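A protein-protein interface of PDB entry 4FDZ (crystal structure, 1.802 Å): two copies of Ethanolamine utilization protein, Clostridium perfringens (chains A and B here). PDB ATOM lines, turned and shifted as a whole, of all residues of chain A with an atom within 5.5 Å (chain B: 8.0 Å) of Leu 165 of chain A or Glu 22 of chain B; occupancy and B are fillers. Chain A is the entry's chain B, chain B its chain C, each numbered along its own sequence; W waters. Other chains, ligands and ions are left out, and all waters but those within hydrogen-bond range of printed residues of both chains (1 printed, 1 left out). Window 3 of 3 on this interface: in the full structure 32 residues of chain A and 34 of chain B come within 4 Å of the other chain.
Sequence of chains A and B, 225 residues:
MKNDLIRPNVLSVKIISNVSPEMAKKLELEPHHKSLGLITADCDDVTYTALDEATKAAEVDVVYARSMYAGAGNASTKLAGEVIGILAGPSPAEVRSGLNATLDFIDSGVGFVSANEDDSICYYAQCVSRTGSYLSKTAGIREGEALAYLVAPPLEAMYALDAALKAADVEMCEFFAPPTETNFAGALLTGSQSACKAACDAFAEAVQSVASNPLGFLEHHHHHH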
ATOM      1  N   ALA A 160      -9.957 -34.676 -11.301  1.00  0.00           N
ATOM      2  CA  ALA A 160      -9.653 -33.439 -12.019  1.00  0.00           C
ATOM      3  C   ALA A 160      -9.689 -32.208 -11.113  1.00  0.00           C
ATOM      4  O   ALA A 160      -8.969 -31.241 -11.354  1.00  0.00           O
ATOM      5  CB  ALA A 160     -10.612 -33.264 -13.196  1.00  0.00           C
ATOM      6  N   LEU A 161     -10.513 -32.239 -10.066  1.00  0.00           N
ATOM      7  CA  LEU A 161     -10.519 -31.135  -9.108  1.00  0.00           C
ATOM      8  C   LEU A 161      -9.176 -31.074  -8.404  1.00  0.00           C
ATOM      9  O   LEU A 161      -8.602 -30.002  -8.200  1.00  0.00           O
ATOM     10  CB  LEU A 161     -11.632 -31.305  -8.071  1.00  0.00           C
ATOM     11  CG  LEU A 161     -13.034 -30.892  -8.508  1.00  0.00           C
ATOM     12  CD1 LEU A 161     -14.011 -31.222  -7.400  1.00  0.00           C
ATOM     13  CD2 LEU A 161     -13.078 -29.405  -8.849  1.00  0.00           C
ATOM     14  N   ASP A 162      -8.662 -32.238  -8.038  1.00  0.00           N
ATOM     15  CA  ASP A 162      -7.374 -32.276  -7.380  1.00  0.00           C
ATOM     16  C   ASP A 162      -6.304 -31.713  -8.308  1.00  0.00           C
ATOM     17  O   ASP A 162      -5.461 -30.925  -7.883  1.00  0.00           O
ATOM     18  CB  ASP A 162      -7.031 -33.687  -6.926  1.00  0.00           C
ATOM     19  CG  ASP A 162      -5.847 -33.697  -5.993  1.00  0.00           C
ATOM     20  OD1 ASP A 162      -6.022 -33.340  -4.801  1.00  0.00           O
ATOM     21  OD2 ASP A 162      -4.757 -34.032  -6.467  1.00  0.00           O
ATOM     22  N   ALA A 163      -6.354 -32.088  -9.583  1.00  0.00           N
ATOM     23  CA  ALA A 163      -5.419 -31.552 -10.570  1.00  0.00           C
ATOM     24  C   ALA A 163      -5.540 -30.033 -10.717  1.00  0.00           C
ATOM     25  O   ALA A 163      -4.529 -29.321 -10.813  1.00  0.00           O
ATOM     26  CB  ALA A 163      -5.633 -32.228 -11.908  1.00  0.00           C
ATOM     27  N   ALA A 164      -6.774 -29.533 -10.743  1.00  0.00           N
ATOM     28  CA  ALA A 164      -7.006 -28.101 -10.918  1.00  0.00           C
ATOM     29  C   ALA A 164      -6.470 -27.329  -9.716  1.00  0.00           C
ATOM     30  O   ALA A 164      -5.824 -26.287  -9.869  1.00  0.00           O
ATOM     31  CB  ALA A 164      -8.483 -27.821 -11.113  1.00  0.00           C
ATOM     32  N   LEU A 165      -6.740 -27.843  -8.521  1.00  0.00           N
ATOM     33  CA  LEU A 165      -6.284 -27.200  -7.295  1.00  0.00           C
ATOM     34  C   LEU A 165      -4.766 -27.172  -7.222  1.00  0.00           C
ATOM     35  O   LEU A 165      -4.198 -26.229  -6.715  1.00  0.00           O
ATOM     36  CB  LEU A 165      -6.854 -27.909  -6.066  1.00  0.00           C
ATOM     37  CG  LEU A 165      -8.358 -27.711  -5.870  1.00  0.00           C
ATOM     38  CD1 LEU A 165      -8.964 -28.834  -5.037  1.00  0.00           C
ATOM     39  CD2 LEU A 165      -8.626 -26.362  -5.217  1.00  0.00           C
ATOM     40  N   LYS A 166      -4.093 -28.199  -7.713  1.00  0.00           N
ATOM     41  CA  LYS A 166      -2.634 -28.186  -7.672  1.00  0.00           C
ATOM     42  C   LYS A 166      -2.038 -27.263  -8.729  1.00  0.00           C
ATOM     43  O   LYS A 166      -0.970 -26.685  -8.522  1.00  0.00           O
ATOM     44  CB  LYS A 166      -2.096 -29.609  -7.798  1.00  0.00           C
ATOM     45  CG  LYS A 166      -2.475 -30.436  -6.571  1.00  0.00           C
ATOM     46  CD  LYS A 166      -1.941 -31.846  -6.591  1.00  0.00           C
ATOM     47  CE  LYS A 166      -2.182 -32.502  -5.235  1.00  0.00           C
ATOM     48  NZ  LYS A 166      -2.244 -33.964  -5.371  1.00  0.00           N
ATOM     49  N   ALA A 167      -2.739 -27.105  -9.846  1.00  0.00           N
ATOM     50  CA  ALA A 167      -2.188 -26.393 -10.998  1.00  0.00           C
ATOM     51  C   ALA A 167      -2.426 -24.889 -10.946  1.00  0.00           C
ATOM     52  O   ALA A 167      -1.645 -24.109 -11.492  1.00  0.00           O
ATOM     53  CB  ALA A 167      -2.783 -26.959 -12.281  1.00  0.00           C
ATOM     54  N   ALA A 168      -3.502 -24.481 -10.289  1.00  0.00           N
ATOM     55  CA  ALA A 168      -3.975 -23.105 -10.385  1.00  0.00           C
ATOM     56  C   ALA A 168      -4.069 -22.456  -9.011  1.00  0.00           C
ATOM     57  O   ALA A 168      -4.358 -23.121  -8.040  1.00  0.00           O
ATOM     58  CB  ALA A 168      -5.331 -23.077 -11.064  1.00  0.00           C
ATOM     59  N   VAL A 170      -6.045 -21.043  -6.868  1.00  0.00           N
ATOM     60  CA  VAL A 170      -7.466 -20.854  -6.565  1.00  0.00           C
ATOM     61  C   VAL A 170      -7.850 -21.406  -5.183  1.00  0.00           C
ATOM     62  O   VAL A 170      -7.083 -22.151  -4.561  1.00  0.00           O
ATOM     63  CB  VAL A 170      -8.339 -21.553  -7.622  1.00  0.00           C
ATOM     64  CG1 VAL A 170      -8.191 -20.867  -8.977  1.00  0.00           C
ATOM     65  CG2 VAL A 170      -7.969 -23.030  -7.730  1.00  0.00           C
ATOM     66  N   GLU A 171      -9.038 -21.037  -4.713  1.00  0.00           N
ATOM     67  CA  GLU A 171      -9.567 -21.520  -3.443  1.00  0.00           C
ATOM     68  C   GLU A 171     -10.868 -22.263  -3.673  1.00  0.00           C
ATOM     69  O   GLU A 171     -11.617 -21.935  -4.584  1.00  0.00           O
ATOM     70  CB  GLU A 171      -9.833 -20.350  -2.500  1.00  0.00           C
ATOM     71  CG  GLU A 171      -8.615 -19.507  -2.213  1.00  0.00           C
ATOM     72  CD  GLU A 171      -8.915 -18.029  -2.309  1.00  0.00           C
ATOM     73  OE1 GLU A 171      -8.615 -17.431  -3.368  1.00  0.00           O
ATOM     74  OE2 GLU A 171      -9.461 -17.474  -1.330  1.00  0.00           O
ATOM     75  N   MET A 172     -11.143 -23.258  -2.837  1.00  0.00           N
ATOM     76  CA  MET A 172     -12.384 -24.012  -2.931  1.00  0.00           C
ATOM     77  C   MET A 172     -13.539 -23.202  -2.356  1.00  0.00           C
ATOM     78  O   MET A 172     -13.420 -22.638  -1.270  1.00  0.00           O
ATOM     79  CB  MET A 172     -12.250 -25.319  -2.149  1.00  0.00           C
ATOM     80  CG  MET A 172     -13.556 -26.033  -1.872  1.00  0.00           C
ATOM     81  SD  MET A 172     -14.317 -26.740  -3.335  1.00  0.00           S
ATOM     82  CE  MET A 172     -13.137 -28.011  -3.790  1.00  0.00           C
ATOM     83  N   LEU A 189     -14.584 -22.904  -7.832  1.00  0.00           N
ATOM     84  CA  LEU A 189     -13.338 -22.414  -7.256  1.00  0.00           C
ATOM     85  C   LEU A 189     -13.192 -20.940  -7.601  1.00  0.00           C
ATOM     86  O   LEU A 189     -13.672 -20.489  -8.643  1.00  0.00           O
ATOM     87  CB  LEU A 189     -12.129 -23.173  -7.806  1.00  0.00           C
ATOM     88  CG  LEU A 189     -12.250 -24.693  -7.937  1.00  0.00           C
ATOM     89  CD1 LEU A 189     -10.971 -25.302  -8.496  1.00  0.00           C
ATOM     90  CD2 LEU A 189     -12.601 -25.352  -6.610  1.00  0.00           C
ATOM     91  N   VAL B  19      -3.157 -35.661  -1.435  1.00  0.00           N
ATOM     92  CA  VAL B  19      -4.415 -34.972  -1.629  1.00  0.00           C
ATOM     93  C   VAL B  19      -4.281 -33.510  -1.212  1.00  0.00           C
ATOM     94  O   VAL B  19      -3.645 -33.183  -0.207  1.00  0.00           O
ATOM     95  CB  VAL B  19      -5.549 -35.672  -0.843  1.00  0.00           C
ATOM     96  CG1 VAL B  19      -5.266 -35.653   0.653  1.00  0.00           C
ATOM     97  CG2 VAL B  19      -6.889 -35.034  -1.156  1.00  0.00           C
ATOM     98  N   SER B  20      -4.864 -32.624  -2.012  1.00  0.00           N
ATOM     99  CA  SER B  20      -4.839 -31.211  -1.696  1.00  0.00           C
ATOM    100  C   SER B  20      -5.593 -30.956  -0.400  1.00  0.00           C
ATOM    101  O   SER B  20      -6.567 -31.651  -0.095  1.00  0.00           O
ATOM    102  CB  SER B  20      -5.477 -30.419  -2.832  1.00  0.00           C
ATOM    103  OG  SER B  20      -6.813 -30.841  -3.040  1.00  0.00           O
ATOM    104  N   PRO B  21      -5.164 -29.946   0.361  1.00  0.00           N
ATOM    105  CA  PRO B  21      -5.841 -29.603   1.612  1.00  0.00           C
ATOM    106  C   PRO B  21      -7.282 -29.185   1.372  1.00  0.00           C
ATOM    107  O   PRO B  21      -8.144 -29.424   2.222  1.00  0.00           O
ATOM    108  CB  PRO B  21      -5.033 -28.410   2.135  1.00  0.00           C
ATOM    109  CG  PRO B  21      -3.755 -28.458   1.424  1.00  0.00           C
ATOM    110  CD  PRO B  21      -4.029 -29.051   0.092  1.00  0.00           C
ATOM    111  N   GLU B  22      -7.538 -28.563   0.225  1.00  0.00           N
ATOM    112  CA  GLU B  22      -8.888 -28.119  -0.113  1.00  0.00           C
ATOM    113  C   GLU B  22      -9.843 -29.303  -0.244  1.00  0.00           C
ATOM    114  O   GLU B  22     -10.959 -29.271   0.275  1.00  0.00           O
ATOM    115  CB  GLU B  22      -8.886 -27.305  -1.411  1.00  0.00           C
ATOM    116  CG  GLU B  22      -8.049 -26.036  -1.357  1.00  0.00           C
ATOM    117  CD  GLU B  22      -6.627 -26.241  -1.854  1.00  0.00           C
ATOM    118  OE1 GLU B  22      -6.195 -27.414  -1.983  1.00  0.00           O
ATOM    119  OE2 GLU B  22      -5.943 -25.226  -2.121  1.00  0.00           O
ATOM    120  N   MET B  23      -9.417 -30.348  -0.946  1.00  0.00           N
ATOM    121  CA  MET B  23     -10.232 -31.551  -1.099  1.00  0.00           C
ATOM    122  C   MET B  23     -10.313 -32.313   0.217  1.00  0.00           C
ATOM    123  O   MET B  23     -11.360 -32.856   0.568  1.00  0.00           O
ATOM    124  CB  MET B  23      -9.661 -32.475  -2.180  1.00  0.00           C
ATOM    125  CG  MET B  23      -9.773 -31.930  -3.600  1.00  0.00           C
ATOM    126  SD  MET B  23     -11.491 -31.822  -4.153  1.00  0.00           S
ATOM    127  CE  MET B  23     -11.863 -33.545  -4.472  1.00  0.00           C
ATOM    128  N   ALA B  24      -9.198 -32.376   0.934  1.00  0.00           N
ATOM    129  CA  ALA B  24      -9.186 -33.080   2.209  1.00  0.00           C
ATOM    130  C   ALA B  24     -10.276 -32.519   3.115  1.00  0.00           C
ATOM    131  O   ALA B  24     -10.975 -33.263   3.801  1.00  0.00           O
ATOM    132  CB  ALA B  24      -7.830 -32.955   2.872  1.00  0.00           C
ATOM    133  N   LYS B  25     -10.419 -31.198   3.104  1.00  0.00           N
ATOM    134  CA  LYS B  25     -11.404 -30.521   3.937  1.00  0.00           C
ATOM    135  C   LYS B  25     -12.845 -30.837   3.515  1.00  0.00           C
ATOM    136  O   LYS B  25     -13.689 -31.150   4.361  1.00  0.00           O
ATOM    137  CB  LYS B  25     -11.147 -29.011   3.904  1.00  0.00           C
ATOM    138  CG  LYS B  25     -12.068 -28.196   4.790  1.00  0.00           C
ATOM    139  CD  LYS B  25     -11.569 -26.755   4.912  1.00  0.00           C
ATOM    140  CE  LYS B  25     -12.433 -25.933   5.863  1.00  0.00           C
ATOM    141  NZ  LYS B  25     -11.795 -24.622   6.194  1.00  0.00           N
ATOM    142  N   LYS B  26     -13.131 -30.778   2.215  1.00  0.00           N
ATOM    143  CA  LYS B  26     -14.482 -31.064   1.744  1.00  0.00           C
ATOM    144  C   LYS B  26     -14.876 -32.532   1.918  1.00  0.00           C
ATOM    145  O   LYS B  26     -16.061 -32.842   2.051  1.00  0.00           O
ATOM    146  CB  LYS B  26     -14.651 -30.641   0.281  1.00  0.00           C
ATOM    147  CG  LYS B  26     -14.664 -29.124   0.092  1.00  0.00           C
ATOM    148  CD  LYS B  26     -15.881 -28.466   0.738  1.00  0.00           C
ATOM    149  CE  LYS B  26     -15.846 -26.954   0.551  1.00  0.00           C
ATOM    150  NZ  LYS B  26     -17.002 -26.256   1.198  1.00  0.00           N
ATOM    151  N   LEU B  27     -13.890 -33.427   1.913  1.00  0.00           N
ATOM    152  CA  LEU B  27     -14.141 -34.853   2.113  1.00  0.00           C
ATOM    153  C   LEU B  27     -14.051 -35.249   3.587  1.00  0.00           C
ATOM    154  O   LEU B  27     -14.271 -36.413   3.945  1.00  0.00           O
ATOM    155  CB  LEU B  27     -13.154 -35.680   1.287  1.00  0.00           C
ATOM    156  CG  LEU B  27     -13.308 -35.568  -0.232  1.00  0.00           C
ATOM    157  CD1 LEU B  27     -12.206 -36.333  -0.939  1.00  0.00           C
ATOM    158  CD2 LEU B  27     -14.675 -36.081  -0.658  1.00  0.00           C
ATOM    159  N   GLU B  28     -13.740 -34.277   4.436  1.00  0.00           N
ATOM    160  CA  GLU B  28     -13.694 -34.481   5.878  1.00  0.00           C
ATOM    161  C   GLU B  28     -12.706 -35.588   6.254  1.00  0.00           C
ATOM    162  O   GLU B  28     -12.985 -36.434   7.111  1.00  0.00           O
ATOM    163  CB  GLU B  28     -15.098 -34.792   6.422  1.00  0.00           C
ATOM    164  CG  GLU B  28     -16.105 -33.661   6.207  1.00  0.00           C
ATOM    165  CD  GLU B  28     -17.468 -33.940   6.826  1.00  0.00           C
ATOM    166  OE1 GLU B  28     -17.861 -35.122   6.928  1.00  0.00           O
ATOM    167  OE2 GLU B  28     -18.148 -32.969   7.209  1.00  0.00           O
ATOM    168  N   LEU B  29     -11.539 -35.558   5.616  1.00  0.00           N
ATOM    169  CA  LEU B  29     -10.495 -36.549   5.874  1.00  0.00           C
ATOM    170  C   LEU B  29      -9.808 -36.336   7.219  1.00  0.00           C
ATOM    171  O   LEU B  29      -9.758 -35.217   7.734  1.00  0.00           O
ATOM    172  CB  LEU B  29      -9.430 -36.480   4.783  1.00  0.00           C
ATOM    173  CG  LEU B  29      -9.909 -36.673   3.345  1.00  0.00           C
ATOM    174  CD1 LEU B  29      -8.721 -36.659   2.414  1.00  0.00           C
ATOM    175  CD2 LEU B  29     -10.689 -37.977   3.220  1.00  0.00           C
HETATM  176  O   HOH W   1      -3.919 -27.334  -3.613  1.00  0.00           O
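Printed residues of chain A within 4 Å of Glu 22 of chain B: Leu 165 and Met 172. No residue of chain B comes within 4 Å of Ala 164 of chain A. Printed residues of chain B within 4 Å of Met 172 of chain A: Glu 22 and Lys 26. Printed residues of chain A within 4 Å of Val 19 of chain B: Asp 162. Printed residues of chain B within 4 Å of Leu 161 of chain A: Met 23. Of the printed residues of chain A, Met 23 of chain B touches Leu 161 and Leu 165. Printed residues of chain A within 4 Å of Lys 26 of chain B: Met 172. The nearest residue of chain A that does not touch Glu 22 of chain B is Val 170 of chain A (4.1 Å). The nearest printed residue of chain B that does not touch Leu 161 of chain A is Ser 20 of chain B (5.5 Å).
Of the 13 printed residues of chain A, 4 touch a printed residue of chain B. Hydrophobic or aromatic side chains of chain B within 4 Å of the printed part of chain A: Met 23. Among the printed residues, no Asp or Glu carboxylate lies within 4 Å of a Lys or Arg side-chain nitrogen of the other chain.
Among the printed residues, merely in contact across the chains: Leu 161 of chain A with Met 23 of chain B (3.95 Å), Asp 162 of chain A with Val 19 of chain B (3.9 Å), Leu 165 of chain A with Ser 20 of chain B (3.6 Å), Leu 165 of chain A with Glu 22 of chain B (3.9 Å), Leu 165 of chain A with Met 23 of chain B (3.5 Å), Met 172 of chain A with Glu 22 of chain B (3.98 Å) and Met 172 of chain A with Lys 26 of chain B (3.5 Å).
Water W1 lies within hydrogen-bond range of OE1 of Glu 22 of chain B and O of Leu 165 of chain A.
No position is printed for both chains.
OD1 of Asp 162 of chain A lies within hydrogen-bond range of N of Ser 20 of chain B (3.1 Å).
The backbone NH of Met 23 of chain B sits close to the side-chain hydroxyl of Ser 20 of chain B. OD2 of Asp 162 of chain A is in salt-bridge range of NZ of Lys 166 of chain A, 2.7 Å away.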
